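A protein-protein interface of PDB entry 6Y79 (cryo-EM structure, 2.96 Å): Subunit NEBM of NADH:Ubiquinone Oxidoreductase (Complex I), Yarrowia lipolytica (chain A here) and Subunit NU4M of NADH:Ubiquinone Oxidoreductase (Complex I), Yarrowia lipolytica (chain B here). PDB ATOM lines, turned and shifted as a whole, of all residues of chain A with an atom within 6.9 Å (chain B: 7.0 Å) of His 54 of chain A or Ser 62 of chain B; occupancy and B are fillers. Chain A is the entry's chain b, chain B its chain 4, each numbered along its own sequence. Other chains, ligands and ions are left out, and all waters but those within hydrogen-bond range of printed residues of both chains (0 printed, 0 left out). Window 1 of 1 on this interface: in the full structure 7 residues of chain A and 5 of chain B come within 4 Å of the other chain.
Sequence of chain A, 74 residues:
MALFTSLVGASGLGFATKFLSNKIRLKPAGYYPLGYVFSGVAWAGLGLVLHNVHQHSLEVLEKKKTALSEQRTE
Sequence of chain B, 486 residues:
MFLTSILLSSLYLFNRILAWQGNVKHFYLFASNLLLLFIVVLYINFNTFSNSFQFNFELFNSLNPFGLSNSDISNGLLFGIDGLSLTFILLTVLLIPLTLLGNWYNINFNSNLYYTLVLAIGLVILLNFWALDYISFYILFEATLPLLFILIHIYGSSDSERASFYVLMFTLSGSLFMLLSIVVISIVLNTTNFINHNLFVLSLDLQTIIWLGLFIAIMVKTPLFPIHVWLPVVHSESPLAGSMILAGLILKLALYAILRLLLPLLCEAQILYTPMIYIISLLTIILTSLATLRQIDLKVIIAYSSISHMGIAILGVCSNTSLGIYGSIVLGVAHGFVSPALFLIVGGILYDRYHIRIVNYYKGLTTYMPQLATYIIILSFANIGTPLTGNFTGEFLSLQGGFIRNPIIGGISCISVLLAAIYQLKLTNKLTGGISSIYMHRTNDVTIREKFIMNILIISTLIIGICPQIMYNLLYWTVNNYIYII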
ATOM      1  N   ALA A   2     -15.273  10.816  16.482  1.00  0.00           N
ATOM      2  CA  ALA A   2     -14.497  11.782  15.716  1.00  0.00           C
ATOM      3  C   ALA A   2     -15.247  13.099  15.566  1.00  0.00           C
ATOM      4  O   ALA A   2     -16.470  13.126  15.487  1.00  0.00           O
ATOM      5  CB  ALA A   2     -14.145  11.216  14.351  1.00  0.00           C
ATOM      6  N   SER A   6     -18.651  14.157  12.745  1.00  0.00           N
ATOM      7  CA  SER A   6     -19.768  14.893  13.327  1.00  0.00           C
ATOM      8  C   SER A   6     -20.055  16.169  12.551  1.00  0.00           C
ATOM      9  O   SER A   6     -21.221  16.490  12.280  1.00  0.00           O
ATOM     10  CB  SER A   6     -19.467  15.223  14.786  1.00  0.00           C
ATOM     11  OG  SER A   6     -19.290  14.044  15.549  1.00  0.00           O
ATOM     12  N   VAL A  49     -21.290  22.601  18.828  1.00  0.00           N
ATOM     13  CA  VAL A  49     -21.743  22.867  20.194  1.00  0.00           C
ATOM     14  C   VAL A  49     -22.065  21.565  20.918  1.00  0.00           C
ATOM     15  O   VAL A  49     -21.607  21.332  22.046  1.00  0.00           O
ATOM     16  CB  VAL A  49     -22.955  23.817  20.173  1.00  0.00           C
ATOM     17  CG1 VAL A  49     -23.614  23.890  21.535  1.00  0.00           C
ATOM     18  CG2 VAL A  49     -22.528  25.194  19.733  1.00  0.00           C
ATOM     19  N   LEU A  50     -22.816  20.679  20.257  1.00  0.00           N
ATOM     20  CA  LEU A  50     -23.241  19.430  20.881  1.00  0.00           C
ATOM     21  C   LEU A  50     -22.060  18.502  21.150  1.00  0.00           C
ATOM     22  O   LEU A  50     -22.010  17.832  22.194  1.00  0.00           O
ATOM     23  CB  LEU A  50     -24.274  18.758  19.988  1.00  0.00           C
ATOM     24  CG  LEU A  50     -25.232  17.744  20.587  1.00  0.00           C
ATOM     25  CD1 LEU A  50     -25.839  18.282  21.862  1.00  0.00           C
ATOM     26  CD2 LEU A  50     -26.310  17.468  19.575  1.00  0.00           C
ATOM     27  N   HIS A  51     -21.071  18.502  20.250  1.00  0.00           N
ATOM     28  CA  HIS A  51     -19.868  17.703  20.442  1.00  0.00           C
ATOM     29  C   HIS A  51     -19.047  18.199  21.622  1.00  0.00           C
ATOM     30  O   HIS A  51     -18.545  17.393  22.417  1.00  0.00           O
ATOM     31  CB  HIS A  51     -19.028  17.726  19.170  1.00  0.00           C
ATOM     32  CG  HIS A  51     -17.872  16.781  19.196  1.00  0.00           C
ATOM     33  ND1 HIS A  51     -16.619  17.149  19.633  1.00  0.00           N
ATOM     34  CD2 HIS A  51     -17.782  15.477  18.850  1.00  0.00           C
ATOM     35  CE1 HIS A  51     -15.806  16.112  19.554  1.00  0.00           C
ATOM     36  NE2 HIS A  51     -16.486  15.085  19.082  1.00  0.00           N
ATOM     37  N   ASN A  52     -18.916  19.522  21.765  1.00  0.00           N
ATOM     38  CA  ASN A  52     -18.128  20.063  22.868  1.00  0.00           C
ATOM     39  C   ASN A  52     -18.809  19.834  24.211  1.00  0.00           C
ATOM     40  O   ASN A  52     -18.136  19.584  25.222  1.00  0.00           O
ATOM     41  CB  ASN A  52     -17.867  21.544  22.639  1.00  0.00           C
ATOM     42  CG  ASN A  52     -16.930  21.788  21.485  1.00  0.00           C
ATOM     43  OD1 ASN A  52     -15.968  21.050  21.288  1.00  0.00           O
ATOM     44  ND2 ASN A  52     -17.204  22.824  20.711  1.00  0.00           N
ATOM     45  N   VAL A  53     -20.142  19.876  24.235  1.00  0.00           N
ATOM     46  CA  VAL A  53     -20.857  19.648  25.487  1.00  0.00           C
ATOM     47  C   VAL A  53     -20.771  18.184  25.901  1.00  0.00           C
ATOM     48  O   VAL A  53     -20.570  17.875  27.086  1.00  0.00           O
ATOM     49  CB  VAL A  53     -22.303  20.148  25.347  1.00  0.00           C
ATOM     50  CG1 VAL A  53     -23.141  19.782  26.543  1.00  0.00           C
ATOM     51  CG2 VAL A  53     -22.267  21.630  25.213  1.00  0.00           C
ATOM     52  N   HIS A  54     -20.839  17.263  24.935  1.00  0.00           N
ATOM     53  CA  HIS A  54     -20.639  15.853  25.265  1.00  0.00           C
ATOM     54  C   HIS A  54     -19.213  15.570  25.732  1.00  0.00           C
ATOM     55  O   HIS A  54     -18.999  14.738  26.623  1.00  0.00           O
ATOM     56  CB  HIS A  54     -20.976  14.979  24.068  1.00  0.00           C
ATOM     57  CG  HIS A  54     -20.901  13.519  24.367  1.00  0.00           C
ATOM     58  ND1 HIS A  54     -19.821  12.742  24.020  1.00  0.00           N
ATOM     59  CD2 HIS A  54     -21.770  12.698  24.998  1.00  0.00           C
ATOM     60  CE1 HIS A  54     -20.031  11.502  24.415  1.00  0.00           C
ATOM     61  NE2 HIS A  54     -21.207  11.448  25.012  1.00  0.00           N
ATOM     62  N   GLN A  55     -18.233  16.270  25.157  1.00  0.00           N
ATOM     63  CA  GLN A  55     -16.839  16.100  25.559  1.00  0.00           C
ATOM     64  C   GLN A  55     -16.606  16.556  26.996  1.00  0.00           C
ATOM     65  O   GLN A  55     -15.976  15.840  27.793  1.00  0.00           O
ATOM     66  CB  GLN A  55     -15.951  16.866  24.584  1.00  0.00           C
ATOM     67  CG  GLN A  55     -14.470  16.765  24.832  1.00  0.00           C
ATOM     68  CD  GLN A  55     -13.691  17.623  23.861  1.00  0.00           C
ATOM     69  OE1 GLN A  55     -14.264  18.214  22.948  1.00  0.00           O
ATOM     70  NE2 GLN A  55     -12.380  17.709  24.060  1.00  0.00           N
ATOM     71  N   HIS A  56     -17.122  17.742  27.349  1.00  0.00           N
ATOM     72  CA  HIS A  56     -16.990  18.239  28.718  1.00  0.00           C
ATOM     73  C   HIS A  56     -17.708  17.331  29.704  1.00  0.00           C
ATOM     74  O   HIS A  56     -17.244  17.127  30.831  1.00  0.00           O
ATOM     75  CB  HIS A  56     -17.542  19.658  28.813  1.00  0.00           C
ATOM     76  CG  HIS A  56     -17.384  20.268  30.166  1.00  0.00           C
ATOM     77  ND1 HIS A  56     -18.360  20.201  31.136  1.00  0.00           N
ATOM     78  CD2 HIS A  56     -16.341  20.919  30.727  1.00  0.00           C
ATOM     79  CE1 HIS A  56     -17.933  20.803  32.230  1.00  0.00           C
ATOM     80  NE2 HIS A  56     -16.710  21.246  32.007  1.00  0.00           N
ATOM     81  N   SER A  57     -18.826  16.750  29.271  1.00  0.00           N
ATOM     82  CA  SER A  57     -19.603  15.807  30.068  1.00  0.00           C
ATOM     83  C   SER A  57     -18.853  14.520  30.370  1.00  0.00           C
ATOM     84  O   SER A  57     -18.923  13.993  31.492  1.00  0.00           O
ATOM     85  CB  SER A  57     -20.860  15.489  29.292  1.00  0.00           C
ATOM     86  OG  SER A  57     -21.633  16.687  29.155  1.00  0.00           O
ATOM     87  N   LEU A  58     -18.149  13.991  29.366  1.00  0.00           N
ATOM     88  CA  LEU A  58     -17.308  12.819  29.581  1.00  0.00           C
ATOM     89  C   LEU A  58     -16.146  13.123  30.516  1.00  0.00           C
ATOM     90  O   LEU A  58     -15.738  12.266  31.316  1.00  0.00           O
ATOM     91  CB  LEU A  58     -16.773  12.318  28.258  1.00  0.00           C
ATOM     92  CG  LEU A  58     -17.736  11.699  27.263  1.00  0.00           C
ATOM     93  CD1 LEU A  58     -16.925  11.340  26.073  1.00  0.00           C
ATOM     94  CD2 LEU A  58     -18.387  10.481  27.854  1.00  0.00           C
ATOM     95  N   GLU A  59     -15.592  14.334  30.421  1.00  0.00           N
ATOM     96  CA  GLU A  59     -14.499  14.697  31.321  1.00  0.00           C
ATOM     97  C   GLU A  59     -14.977  14.828  32.765  1.00  0.00           C
ATOM     98  O   GLU A  59     -14.266  14.423  33.695  1.00  0.00           O
ATOM     99  CB  GLU A  59     -13.832  15.980  30.838  1.00  0.00           C
ATOM    100  CG  GLU A  59     -13.088  15.773  29.541  1.00  0.00           C
ATOM    101  CD  GLU A  59     -12.613  17.061  28.924  1.00  0.00           C
ATOM    102  OE1 GLU A  59     -12.886  18.132  29.499  1.00  0.00           O
ATOM    103  OE2 GLU A  59     -11.971  16.999  27.856  1.00  0.00           O
ATOM    104  N   GLU B  58     -20.962  -0.818  14.373  1.00  0.00           N
ATOM    105  CA  GLU B  58     -21.835  -0.092  15.282  1.00  0.00           C
ATOM    106  C   GLU B  58     -22.186   1.255  14.678  1.00  0.00           C
ATOM    107  O   GLU B  58     -21.311   1.958  14.171  1.00  0.00           O
ATOM    108  CB  GLU B  58     -21.173   0.105  16.640  1.00  0.00           C
ATOM    109  CG  GLU B  58     -22.095   0.674  17.686  1.00  0.00           C
ATOM    110  CD  GLU B  58     -21.403   0.902  19.005  1.00  0.00           C
ATOM    111  OE1 GLU B  58     -20.201   0.584  19.112  1.00  0.00           O
ATOM    112  OE2 GLU B  58     -22.058   1.405  19.937  1.00  0.00           O
ATOM    113  N   LEU B  59     -23.463   1.608  14.729  1.00  0.00           N
ATOM    114  CA  LEU B  59     -23.945   2.894  14.258  1.00  0.00           C
ATOM    115  C   LEU B  59     -24.481   3.695  15.431  1.00  0.00           C
ATOM    116  O   LEU B  59     -24.993   3.129  16.396  1.00  0.00           O
ATOM    117  CB  LEU B  59     -25.046   2.731  13.211  1.00  0.00           C
ATOM    118  CG  LEU B  59     -24.673   2.218  11.828  1.00  0.00           C
ATOM    119  CD1 LEU B  59     -25.870   2.335  10.928  1.00  0.00           C
ATOM    120  CD2 LEU B  59     -23.510   2.987  11.262  1.00  0.00           C
ATOM    121  N   PHE B  60     -24.323   5.019  15.337  1.00  0.00           N
ATOM    122  CA  PHE B  60     -24.907   5.993  16.268  1.00  0.00           C
ATOM    123  C   PHE B  60     -24.410   5.803  17.699  1.00  0.00           C
ATOM    124  O   PHE B  60     -25.171   5.907  18.659  1.00  0.00           O
ATOM    125  CB  PHE B  60     -26.434   5.968  16.203  1.00  0.00           C
ATOM    126  CG  PHE B  60     -26.959   6.141  14.824  1.00  0.00           C
ATOM    127  CD1 PHE B  60     -26.637   7.266  14.111  1.00  0.00           C
ATOM    128  CD2 PHE B  60     -27.749   5.179  14.229  1.00  0.00           C
ATOM    129  CE1 PHE B  60     -27.090   7.441  12.832  1.00  0.00           C
ATOM    130  CE2 PHE B  60     -28.211   5.351  12.949  1.00  0.00           C
ATOM    131  CZ  PHE B  60     -27.884   6.483  12.253  1.00  0.00           C
ATOM    132  N   ASN B  61     -23.121   5.515  17.839  1.00  0.00           N
ATOM    133  CA  ASN B  61     -22.465   5.569  19.132  1.00  0.00           C
ATOM    134  C   ASN B  61     -22.318   7.026  19.551  1.00  0.00           C
ATOM    135  O   ASN B  61     -22.398   7.932  18.733  1.00  0.00           O
ATOM    136  CB  ASN B  61     -21.102   4.883  19.055  1.00  0.00           C
ATOM    137  CG  ASN B  61     -20.568   4.488  20.406  1.00  0.00           C
ATOM    138  OD1 ASN B  61     -21.208   4.700  21.415  1.00  0.00           O
ATOM    139  ND2 ASN B  61     -19.384   3.909  20.427  1.00  0.00           N
ATOM    140  N   SER B  62     -22.112   7.259  20.843  1.00  0.00           N
ATOM    141  CA  SER B  62     -22.020   8.639  21.313  1.00  0.00           C
ATOM    142  C   SER B  62     -20.681   9.263  20.941  1.00  0.00           C
ATOM    143  O   SER B  62     -20.615  10.442  20.584  1.00  0.00           O
ATOM    144  CB  SER B  62     -22.252   8.702  22.818  1.00  0.00           C
ATOM    145  OG  SER B  62     -21.237   8.026  23.523  1.00  0.00           O
ATOM    146  N   LEU B  63     -19.601   8.485  20.993  1.00  0.00           N
ATOM    147  CA  LEU B  63     -18.291   9.015  20.630  1.00  0.00           C
ATOM    148  C   LEU B  63     -18.168   9.327  19.142  1.00  0.00           C
ATOM    149  O   LEU B  63     -17.352  10.172  18.765  1.00  0.00           O
ATOM    150  CB  LEU B  63     -17.199   8.037  21.050  1.00  0.00           C
ATOM    151  CG  LEU B  63     -16.939   8.009  22.553  1.00  0.00           C
ATOM    152  CD1 LEU B  63     -15.842   7.026  22.894  1.00  0.00           C
ATOM    153  CD2 LEU B  63     -16.558   9.384  23.001  1.00  0.00           C
ATOM    154  N   ASN B  64     -18.962   8.673  18.296  1.00  0.00           N
ATOM    155  CA  ASN B  64     -19.004   8.966  16.866  1.00  0.00           C
ATOM    156  C   ASN B  64     -20.431   8.733  16.393  1.00  0.00           C
ATOM    157  O   ASN B  64     -20.798   7.611  16.025  1.00  0.00           O
ATOM    158  CB  ASN B  64     -18.019   8.092  16.092  1.00  0.00           C
ATOM    159  CG  ASN B  64     -17.672   8.662  14.737  1.00  0.00           C
ATOM    160  OD1 ASN B  64     -18.322   9.584  14.250  1.00  0.00           O
ATOM    161  ND2 ASN B  64     -16.642   8.110  14.117  1.00  0.00           N
ATOM    162  N   PRO B  65     -21.276   9.770  16.410  1.00  0.00           N
ATOM    163  CA  PRO B  65     -22.674   9.576  15.988  1.00  0.00           C
ATOM    164  C   PRO B  65     -22.845   9.374  14.498  1.00  0.00           C
ATOM    165  O   PRO B  65     -23.789   8.693  14.088  1.00  0.00           O
ATOM    166  CB  PRO B  65     -23.370  10.857  16.470  1.00  0.00           C
ATOM    167  CG  PRO B  65     -22.469  11.421  17.496  1.00  0.00           C
ATOM    168  CD  PRO B  65     -21.085  11.077  17.052  1.00  0.00           C
ATOM    169  N   SER B  69     -17.519   2.987  14.971  1.00  0.00           N
ATOM    170  CA  SER B  69     -17.211   3.175  16.379  1.00  0.00           C
ATOM    171  C   SER B  69     -16.080   2.259  16.818  1.00  0.00           C
ATOM    172  O   SER B  69     -16.188   1.035  16.702  1.00  0.00           O
ATOM    173  CB  SER B  69     -18.449   2.919  17.233  1.00  0.00           C
ATOM    174  OG  SER B  69     -18.132   3.021  18.602  1.00  0.00           O
ATOM    175  N   SER B  71     -14.567   1.984  20.302  1.00  0.00           N
ATOM    176  CA  SER B  71     -14.760   2.540  21.634  1.00  0.00           C
ATOM    177  C   SER B  71     -14.674   1.471  22.715  1.00  0.00           C
ATOM    178  O   SER B  71     -14.853   0.276  22.468  1.00  0.00           O
ATOM    179  CB  SER B  71     -16.101   3.267  21.739  1.00  0.00           C
ATOM    180  OG  SER B  71     -16.160   4.341  20.823  1.00  0.00           O
ATOM    181  N   ILE B  73     -16.791   1.734  25.142  1.00  0.00           N
ATOM    182  CA  ILE B  73     -18.161   1.732  25.629  1.00  0.00           C
ATOM    183  C   ILE B  73     -19.078   1.857  24.422  1.00  0.00           C
ATOM    184  O   ILE B  73     -18.763   2.564  23.458  1.00  0.00           O
ATOM    185  CB  ILE B  73     -18.389   2.848  26.675  1.00  0.00           C
ATOM    186  CG1 ILE B  73     -19.653   2.598  27.465  1.00  0.00           C
ATOM    187  CG2 ILE B  73     -18.409   4.266  26.083  1.00  0.00           C
ATOM    188  CD1 ILE B  73     -19.692   3.402  28.705  1.00  0.00           C
ATOM    189  N   SER B  74     -20.153   1.088  24.416  1.00  0.00           N
ATOM    190  CA  SER B  74     -20.971   0.961  23.225  1.00  0.00           C
ATOM    191  C   SER B  74     -22.428   1.054  23.617  1.00  0.00           C
ATOM    192  O   SER B  74     -22.933   0.195  24.344  1.00  0.00           O
ATOM    193  CB  SER B  74     -20.694  -0.351  22.509  1.00  0.00           C
ATOM    194  OG  SER B  74     -21.089  -1.436  23.320  1.00  0.00           O
ATOM    195  N   ASN B  75     -23.100   2.092  23.127  1.00  0.00           N
ATOM    196  CA  ASN B  75     -24.520   2.257  23.371  1.00  0.00           C
ATOM    197  C   ASN B  75     -25.297   2.592  22.106  1.00  0.00           C
ATOM    198  O   ASN B  75     -26.432   3.065  22.203  1.00  0.00           O
ATOM    199  CB  ASN B  75     -24.765   3.321  24.445  1.00  0.00           C
ATOM    200  CG  ASN B  75     -24.027   4.619  24.178  1.00  0.00           C
ATOM    201  OD1 ASN B  75     -23.398   4.794  23.147  1.00  0.00           O
ATOM    202  ND2 ASN B  75     -24.112   5.540  25.120  1.00  0.00           N
ATOM    203  N   GLY B  76     -24.729   2.357  20.929  1.00  0.00           N
ATOM    204  CA  GLY B  76     -25.462   2.564  19.699  1.00  0.00           C
ATOM    205  C   GLY B  76     -26.228   1.337  19.254  1.00  0.00           C
ATOM    206  O   GLY B  76     -26.750   0.587  20.080  1.00  0.00           O
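Among the printed residues, merely in contact across the chains: Leu 58 of chain A with Leu 63 of chain B (3.7 Å), Ala 2 of chain A with Asn 64 of chain B (3.7 Å), His 54 of chain A with Ser 62 of chain B (3.7 Å) and Ser 6 of chain A with Pro 65 of chain B (3.8 Å).
Of the 13 printed residues of chain A, 4 touch a printed residue of chain B.
Along chain A the printed residues that touch a printed residue of chain B span positions 2 to 58.
Hydrophobic or aromatic side chains of chain B that line the printed part of chain A: Leu 63 and Pro 65.
Among the printed residues, 5 pairs touch across the chains.
O of Ala 2 of chain A is in hydrogen-bond range of OG of Ser 6 of chain A, 3.0 Å away.
Of the printed residues of chain B, Ala 2 of chain A touches Leu 63 and Asn 64.
Of chain B, only Ser 62 (3.7 Å) comes within 4 Å of His 54 of chain A.
Of the printed residues of chain B, Leu 58 of chain A touches Leu 63 (3.7 Å).
Printed residues of chain A within 4 Å of Ser 62 of chain B: His 54.
Of the printed residues of chain A, Leu 63 of chain B touches Ala 2 (3.2 Å) and Leu 58 (3.7 Å).
Of the printed residues of chain A, Asn 64 of chain B touches Ala 2.
Of the printed residues of chain A, Pro 65 of chain B touches Ser 6.
The nearest residue of chain B that does not touch His 54 of chain A is Leu 63 of chain B (4.3 Å).
The backbone NH (N) of Ala 2 of chain A is in hydrogen-bond range of the backbone carbonyl oxygen (O) of Leu 63 of chain B (3.2 Å).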
